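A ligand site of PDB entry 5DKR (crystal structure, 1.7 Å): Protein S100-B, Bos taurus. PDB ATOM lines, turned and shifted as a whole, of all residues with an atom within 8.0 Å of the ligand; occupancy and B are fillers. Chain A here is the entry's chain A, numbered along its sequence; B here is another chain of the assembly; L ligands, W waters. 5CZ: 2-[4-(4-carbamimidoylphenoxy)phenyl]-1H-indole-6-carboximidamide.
Phe 88 touches the ligand.
Met 1 of chain B touches the ligand (CE to C4, 3.4 Å).
Val 9 of chain B touches the ligand.
The backbone carbonyl oxygen of His 43 sits at hydrogen-bond distance from a nitrogen (N12) of the ligand, 2.7 Å away.
A nitrogen (N27) of the ligand is in salt-bridge range of the side-chain carboxylate (OD1) of Asp 13 of chain B (2.7 Å).
N38 of the ligand is in hydrogen-bond range of O of Phe 44, at 2.9 Å.
OE2 of Glu 46 lies within salt-bridge range of N35 of the ligand, at 3.3 Å.
A ring nitrogen (ND1) of His 43 sits at hydrogen-bond distance from the side-chain carboxylate (OE1) of Glu 5 of chain B (2.6 Å).
Water W2 bridges OD1 of Asp 13 of chain B and N27 of the ligand.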
ATOM      1  N   LEU A  41      27.704  -6.081  10.298  1.00  0.00           N
ATOM      2  CA  LEU A  41      27.132  -4.865  10.884  1.00  0.00           C
ATOM      3  C   LEU A  41      25.784  -4.483  10.265  1.00  0.00           C
ATOM      4  O   LEU A  41      25.408  -3.308  10.256  1.00  0.00           O
ATOM      5  CB  LEU A  41      28.104  -3.703  10.745  1.00  0.00           C
ATOM      6  CG  LEU A  41      29.382  -3.897  11.557  1.00  0.00           C
ATOM      7  CD1 LEU A  41      30.429  -2.851  11.212  1.00  0.00           C
ATOM      8  CD2 LEU A  41      29.054  -3.883  13.046  1.00  0.00           C
ATOM      9  N   SER A  42      25.070  -5.483   9.772  1.00  0.00           N
ATOM     10  CA  SER A  42      23.827  -5.254   9.032  1.00  0.00           C
ATOM     11  C   SER A  42      22.709  -4.647   9.892  1.00  0.00           C
ATOM     12  O   SER A  42      21.740  -4.102   9.362  1.00  0.00           O
ATOM     13  CB  SER A  42      23.344  -6.555   8.396  1.00  0.00           C
ATOM     14  OG  SER A  42      22.749  -7.393   9.365  1.00  0.00           O
ATOM     15  N   HIS A  43      22.831  -4.735  11.210  1.00  0.00           N
ATOM     16  CA  HIS A  43      21.875  -4.090  12.099  1.00  0.00           C
ATOM     17  C   HIS A  43      22.315  -2.695  12.558  1.00  0.00           C
ATOM     18  O   HIS A  43      21.528  -2.004  13.201  1.00  0.00           O
ATOM     19  CB  HIS A  43      21.559  -4.961  13.318  1.00  0.00           C
ATOM     20  CG  HIS A  43      21.147  -6.351  12.978  1.00  0.00           C
ATOM     21  ND1 HIS A  43      22.024  -7.417  12.970  1.00  0.00           N
ATOM     22  CD2 HIS A  43      19.943  -6.868  12.632  1.00  0.00           C
ATOM     23  CE1 HIS A  43      21.382  -8.516  12.631  1.00  0.00           C
ATOM     24  NE2 HIS A  43      20.116  -8.219  12.423  1.00  0.00           N
ATOM     25  N   PHE A  44      23.544  -2.291  12.241  1.00  0.00           N
ATOM     26  CA  PHE A  44      24.065  -0.967  12.643  1.00  0.00           C
ATOM     27  C   PHE A  44      24.334  -0.044  11.465  1.00  0.00           C
ATOM     28  O   PHE A  44      24.135   1.168  11.554  1.00  0.00           O
ATOM     29  CB  PHE A  44      25.381  -1.087  13.450  1.00  0.00           C
ATOM     30  CG  PHE A  44      25.230  -1.760  14.784  1.00  0.00           C
ATOM     31  CD1 PHE A  44      24.003  -1.910  15.384  1.00  0.00           C
ATOM     32  CD2 PHE A  44      26.350  -2.249  15.446  1.00  0.00           C
ATOM     33  CE1 PHE A  44      23.882  -2.535  16.619  1.00  0.00           C
ATOM     34  CE2 PHE A  44      26.236  -2.867  16.678  1.00  0.00           C
ATOM     35  CZ  PHE A  44      24.990  -3.011  17.253  1.00  0.00           C
ATOM     36  N   LEU A  45      24.785  -0.578  10.336  1.00  0.00           N
ATOM     37  CA  LEU A  45      25.213   0.226   9.221  1.00  0.00           C
ATOM     38  C   LEU A  45      24.467  -0.186   7.961  1.00  0.00           C
ATOM     39  O   LEU A  45      24.175  -1.332   7.766  1.00  0.00           O
ATOM     40  CB  LEU A  45      26.709   0.084   8.983  1.00  0.00           C
ATOM     41  CG  LEU A  45      27.750   0.528  10.019  1.00  0.00           C
ATOM     42  CD1 LEU A  45      29.178   0.394   9.604  1.00  0.00           C
ATOM     43  CD2 LEU A  45      27.519   1.941  10.427  1.00  0.00           C
ATOM     44  N   GLU A  46      24.157   0.777   7.096  1.00  0.00           N
ATOM     45  CA  GLU A  46      23.471   0.446   5.866  1.00  0.00           C
ATOM     46  C   GLU A  46      24.408  -0.314   4.985  1.00  0.00           C
ATOM     47  O   GLU A  46      25.523   0.012   4.911  1.00  0.00           O
ATOM     48  CB  GLU A  46      23.036   1.710   5.121  1.00  0.00           C
ATOM     49  CG  GLU A  46      22.370   2.742   5.996  1.00  0.00           C
ATOM     50  CD  GLU A  46      20.899   2.480   6.276  1.00  0.00           C
ATOM     51  OE1 GLU A  46      20.351   1.535   5.713  1.00  0.00           O
ATOM     52  OE2 GLU A  46      20.283   3.234   7.041  1.00  0.00           O
ATOM     53  N   GLU A  47      23.872  -1.341   4.329  1.00  0.00           N
ATOM     54  CA  GLU A  47      24.549  -2.148   3.319  1.00  0.00           C
ATOM     55  C   GLU A  47      25.267  -1.330   2.309  1.00  0.00           C
ATOM     56  O   GLU A  47      24.736  -0.431   1.745  1.00  0.00           O
ATOM     57  CB  GLU A  47      23.555  -3.046   2.621  1.00  0.00           C
ATOM     58  CG  GLU A  47      24.149  -4.161   1.797  1.00  0.00           C
ATOM     59  CD  GLU A  47      23.110  -4.989   1.042  1.00  0.00           C
ATOM     60  OE1 GLU A  47      21.944  -4.899   1.323  1.00  0.00           O
ATOM     61  OE2 GLU A  47      23.489  -5.792   0.203  1.00  0.00           O
ATOM     62  N   CYS A  85      26.911   4.177  18.579  1.00  0.00           N
ATOM     63  CA  CYS A  85      25.803   3.453  19.180  1.00  0.00           C
ATOM     64  C   CYS A  85      25.513   3.989  20.578  1.00  0.00           C
ATOM     65  O   CYS A  85      24.352   4.183  20.944  1.00  0.00           O
ATOM     66  CB  CYS A  85      26.095   1.960  19.224  1.00  0.00           C
ATOM     67  SG  CYS A  85      24.758   1.013  19.955  1.00  0.00           S
ATOM     68  N   PHE A  88      23.850   7.477  20.430  1.00  0.00           N
ATOM     69  CA  PHE A  88      22.473   7.314  19.974  1.00  0.00           C
ATOM     70  C   PHE A  88      21.538   7.087  21.156  1.00  0.00           C
ATOM     71  O   PHE A  88      20.481   7.707  21.261  1.00  0.00           O
ATOM     72  CB  PHE A  88      22.395   6.126  19.025  1.00  0.00           C
ATOM     73  CG  PHE A  88      21.002   5.791  18.575  1.00  0.00           C
ATOM     74  CD1 PHE A  88      20.289   4.786  19.202  1.00  0.00           C
ATOM     75  CD2 PHE A  88      20.417   6.474  17.522  1.00  0.00           C
ATOM     76  CE1 PHE A  88      19.008   4.472  18.802  1.00  0.00           C
ATOM     77  CE2 PHE A  88      19.132   6.153  17.091  1.00  0.00           C
ATOM     78  CZ  PHE A  88      18.420   5.155  17.740  1.00  0.00           C
ATOM     79  N   PHE A  89      21.939   6.192  22.047  1.00  0.00           N
ATOM     80  CA  PHE A  89      21.099   5.831  23.177  1.00  0.00           C
ATOM     81  C   PHE A  89      21.210   6.809  24.329  1.00  0.00           C
ATOM     82  O   PHE A  89      20.478   6.707  25.304  1.00  0.00           O
ATOM     83  CB  PHE A  89      21.429   4.412  23.650  1.00  0.00           C
ATOM     84  CG  PHE A  89      20.959   3.341  22.706  1.00  0.00           C
ATOM     85  CD1 PHE A  89      19.606   3.166  22.467  1.00  0.00           C
ATOM     86  CD2 PHE A  89      21.869   2.502  22.075  1.00  0.00           C
ATOM     87  CE1 PHE A  89      19.182   2.194  21.612  1.00  0.00           C
ATOM     88  CE2 PHE A  89      21.445   1.509  21.197  1.00  0.00           C
ATOM     89  CZ  PHE A  89      20.096   1.348  20.969  1.00  0.00           C
ATOM     90  N   MET B   1      21.697 -10.697  16.762  1.00  0.00           N
ATOM     91  CA  MET B   1      22.738  -9.905  16.125  1.00  0.00           C
ATOM     92  C   MET B   1      23.977 -10.735  15.832  1.00  0.00           C
ATOM     93  O   MET B   1      24.144 -11.846  16.355  1.00  0.00           O
ATOM     94  CB  MET B   1      23.122  -8.710  16.998  1.00  0.00           C
ATOM     95  CG  MET B   1      21.989  -8.086  17.756  1.00  0.00           C
ATOM     96  SD  MET B   1      22.395  -6.418  18.273  1.00  0.00           S
ATOM     97  CE  MET B   1      22.460  -5.664  16.661  1.00  0.00           C
ATOM     98  N   GLU B   5      28.365  -7.434  16.394  1.00  0.00           N
ATOM     99  CA  GLU B   5      27.340  -6.572  16.976  1.00  0.00           C
ATOM    100  C   GLU B   5      27.123  -6.849  18.460  1.00  0.00           C
ATOM    101  O   GLU B   5      26.980  -5.918  19.263  1.00  0.00           O
ATOM    102  CB  GLU B   5      26.034  -6.685  16.174  1.00  0.00           C
ATOM    103  CG  GLU B   5      26.100  -5.982  14.844  1.00  0.00           C
ATOM    104  CD  GLU B   5      24.991  -6.369  13.892  1.00  0.00           C
ATOM    105  OE1 GLU B   5      24.380  -7.454  14.062  1.00  0.00           O
ATOM    106  OE2 GLU B   5      24.735  -5.592  12.960  1.00  0.00           O
ATOM    107  N   LYS B   6      27.103  -8.130  18.823  1.00  0.00           N
ATOM    108  CA  LYS B   6      27.004  -8.504  20.223  1.00  0.00           C
ATOM    109  C   LYS B   6      28.198  -7.972  21.020  1.00  0.00           C
ATOM    110  O   LYS B   6      28.056  -7.583  22.180  1.00  0.00           O
ATOM    111  CB  LYS B   6      26.909 -10.017  20.389  1.00  0.00           C
ATOM    112  CG  LYS B   6      25.598 -10.614  19.903  1.00  0.00           C
ATOM    113  CD  LYS B   6      25.573 -12.094  20.256  1.00  0.00           C
ATOM    114  CE  LYS B   6      24.578 -12.873  19.395  1.00  0.00           C
ATOM    115  NZ  LYS B   6      24.969 -14.314  19.321  1.00  0.00           N
ATOM    116  N   VAL B   8      30.009  -5.261  20.353  1.00  0.00           N
ATOM    117  CA  VAL B   8      29.848  -3.821  20.460  1.00  0.00           C
ATOM    118  C   VAL B   8      28.921  -3.452  21.619  1.00  0.00           C
ATOM    119  O   VAL B   8      29.258  -2.620  22.445  1.00  0.00           O
ATOM    120  CB  VAL B   8      29.312  -3.213  19.147  1.00  0.00           C
ATOM    121  CG1 VAL B   8      28.823  -1.782  19.350  1.00  0.00           C
ATOM    122  CG2 VAL B   8      30.397  -3.242  18.074  1.00  0.00           C
ATOM    123  N   VAL B   9      27.749  -4.085  21.671  1.00  0.00           N
ATOM    124  CA  VAL B   9      26.787  -3.751  22.725  1.00  0.00           C
ATOM    125  C   VAL B   9      27.239  -4.246  24.096  1.00  0.00           C
ATOM    126  O   VAL B   9      26.932  -3.614  25.110  1.00  0.00           O
ATOM    127  CB  VAL B   9      25.339  -4.198  22.396  1.00  0.00           C
ATOM    128  CG1 VAL B   9      24.850  -3.510  21.117  1.00  0.00           C
ATOM    129  CG2 VAL B   9      25.234  -5.703  22.250  1.00  0.00           C
ATOM    130  N   ALA B  10      28.010  -5.327  24.143  1.00  0.00           N
ATOM    131  CA  ALA B  10      28.597  -5.782  25.402  1.00  0.00           C
ATOM    132  C   ALA B  10      29.503  -4.717  26.031  1.00  0.00           C
ATOM    133  O   ALA B  10      29.544  -4.574  27.253  1.00  0.00           O
ATOM    134  CB  ALA B  10      29.370  -7.111  25.231  1.00  0.00           C
ATOM    135  N   LEU B  11      30.247  -3.980  25.193  1.00  0.00           N
ATOM    136  CA  LEU B  11      31.153  -2.947  25.691  1.00  0.00           C
ATOM    137  C   LEU B  11      30.338  -1.826  26.358  1.00  0.00           C
ATOM    138  O   LEU B  11      30.702  -1.332  27.423  1.00  0.00           O
ATOM    139  CB  LEU B  11      31.997  -2.358  24.539  1.00  0.00           C
ATOM    140  CG  LEU B  11      32.907  -3.336  23.809  1.00  0.00           C
ATOM    141  CD1 LEU B  11      33.670  -2.625  22.670  1.00  0.00           C
ATOM    142  CD2 LEU B  11      33.857  -4.008  24.782  1.00  0.00           C
ATOM    143  N   ILE B  12      29.243  -1.456  25.718  1.00  0.00           N
ATOM    144  CA  ILE B  12      28.363  -0.413  26.239  1.00  0.00           C
ATOM    145  C   ILE B  12      27.665  -0.926  27.492  1.00  0.00           C
ATOM    146  O   ILE B  12      27.502  -0.185  28.467  1.00  0.00           O
ATOM    147  CB  ILE B  12      27.321   0.037  25.174  1.00  0.00           C
ATOM    148  CG1 ILE B  12      28.041   0.606  23.945  1.00  0.00           C
ATOM    149  CG2 ILE B  12      26.375   1.089  25.723  1.00  0.00           C
ATOM    150  CD1 ILE B  12      27.137   0.737  22.700  1.00  0.00           C
ATOM    151  N   ASP B  13      27.263  -2.197  27.485  1.00  0.00           N
ATOM    152  CA  ASP B  13      26.590  -2.756  28.663  1.00  0.00           C
ATOM    153  C   ASP B  13      27.496  -2.751  29.885  1.00  0.00           C
ATOM    154  O   ASP B  13      27.100  -2.311  30.947  1.00  0.00           O
ATOM    155  CB  ASP B  13      26.128  -4.187  28.398  1.00  0.00           C
ATOM    156  CG  ASP B  13      24.885  -4.258  27.515  1.00  0.00           C
ATOM    157  OD1 ASP B  13      24.304  -3.186  27.224  1.00  0.00           O
ATOM    158  OD2 ASP B  13      24.482  -5.385  27.151  1.00  0.00           O
ATOM    159  N   VAL B  14      28.718  -3.245  29.720  1.00  0.00           N
ATOM    160  CA  VAL B  14      29.624  -3.344  30.866  1.00  0.00           C
ATOM    161  C   VAL B  14      29.995  -1.962  31.398  1.00  0.00           C
ATOM    162  O   VAL B  14      30.076  -1.773  32.614  1.00  0.00           O
ATOM    163  CB  VAL B  14      30.867  -4.223  30.593  1.00  0.00           C
ATOM    164  CG1 VAL B  14      31.866  -3.518  29.680  1.00  0.00           C
ATOM    165  CG2 VAL B  14      31.542  -4.668  31.934  1.00  0.00           C
ATOM    166  N   HIS B  16      28.084   0.666  31.332  1.00  0.00           N
ATOM    167  CA  HIS B  16      26.931   1.183  32.043  1.00  0.00           C
ATOM    168  C   HIS B  16      26.754   0.523  33.389  1.00  0.00           C
ATOM    169  O   HIS B  16      26.291   1.126  34.306  1.00  0.00           O
ATOM    170  CB  HIS B  16      25.639   1.020  31.279  1.00  0.00           C
ATOM    171  CG  HIS B  16      25.479   1.944  30.144  1.00  0.00           C
ATOM    172  ND1 HIS B  16      26.026   3.205  30.110  1.00  0.00           N
ATOM    173  CD2 HIS B  16      24.788   1.816  28.992  1.00  0.00           C
ATOM    174  CE1 HIS B  16      25.726   3.788  28.968  1.00  0.00           C
ATOM    175  NE2 HIS B  16      24.934   2.987  28.292  1.00  0.00           N
HETATM  176  C2  5CZ L   1      19.659  -1.073  16.873  1.00  0.00           C
HETATM  177  C3  5CZ L   1      20.616  -2.078  16.917  1.00  0.00           C
HETATM  178  C7  5CZ L   1      18.603  -1.121  17.748  1.00  0.00           C
HETATM  179  C8  5CZ L   1      19.734   0.046  15.888  1.00  0.00           C
HETATM  180  C9  5CZ L   1      19.196   1.319  16.057  1.00  0.00           C
HETATM  181  C10 5CZ L   1      19.553   1.972  14.841  1.00  0.00           C
HETATM  182  C11 5CZ L   1      20.269   1.141  14.010  1.00  0.00           C
HETATM  183  C20 5CZ L   1      20.009  -4.132  20.845  1.00  0.00           C
HETATM  184  C21 5CZ L   1      20.066  -5.312  21.567  1.00  0.00           C
HETATM  185  C22 5CZ L   1      20.771  -5.362  22.777  1.00  0.00           C
HETATM  186  C24 5CZ L   1      21.362  -3.036  22.543  1.00  0.00           C
HETATM  187  N29 5CZ L   1      22.809  -5.582  24.841  1.00  0.00           N
HETATM  188  C30 5CZ L   1      19.278   3.278  14.442  1.00  0.00           C
HETATM  189  C31 5CZ L   1      19.723   3.733  13.198  1.00  0.00           C
HETATM  190  C32 5CZ L   1      20.454   2.874  12.361  1.00  0.00           C
HETATM  191  C33 5CZ L   1      20.716   1.567  12.766  1.00  0.00           C
HETATM  192  C34 5CZ L   1      20.936   3.333  11.026  1.00  0.00           C
HETATM  193  C4  5CZ L   1      20.506  -3.105  17.853  1.00  0.00           C
HETATM  194  C5  5CZ L   1      19.440  -3.141  18.743  1.00  0.00           C
HETATM  195  C6  5CZ L   1      18.486  -2.141  18.686  1.00  0.00           C
HETATM  196  N12 5CZ L   1      20.359  -0.029  14.686  1.00  0.00           N
HETATM  197  O19 5CZ L   1      19.313  -4.133  19.663  1.00  0.00           O
HETATM  198  C23 5CZ L   1      21.407  -4.232  23.270  1.00  0.00           C
HETATM  199  C25 5CZ L   1      20.657  -2.987  21.333  1.00  0.00           C
HETATM  200  C26 5CZ L   1      22.176  -4.358  24.562  1.00  0.00           C
HETATM  201  N27 5CZ L   1      22.305  -3.395  25.358  1.00  0.00           N
HETATM  202  N35 5CZ L   1      20.097   4.136  10.191  1.00  0.00           N
HETATM  203  N38 5CZ L   1      22.097   3.012  10.637  1.00  0.00           N
HETATM  204  O   HOH W   1      17.002   4.520  10.644  1.00  0.00           O
HETATM  205  O   HOH W   2      23.729  -0.637  26.337  1.00  0.00           O
HETATM  206  O   HOH W   3      22.810  -8.176  23.418  1.00  0.00           O
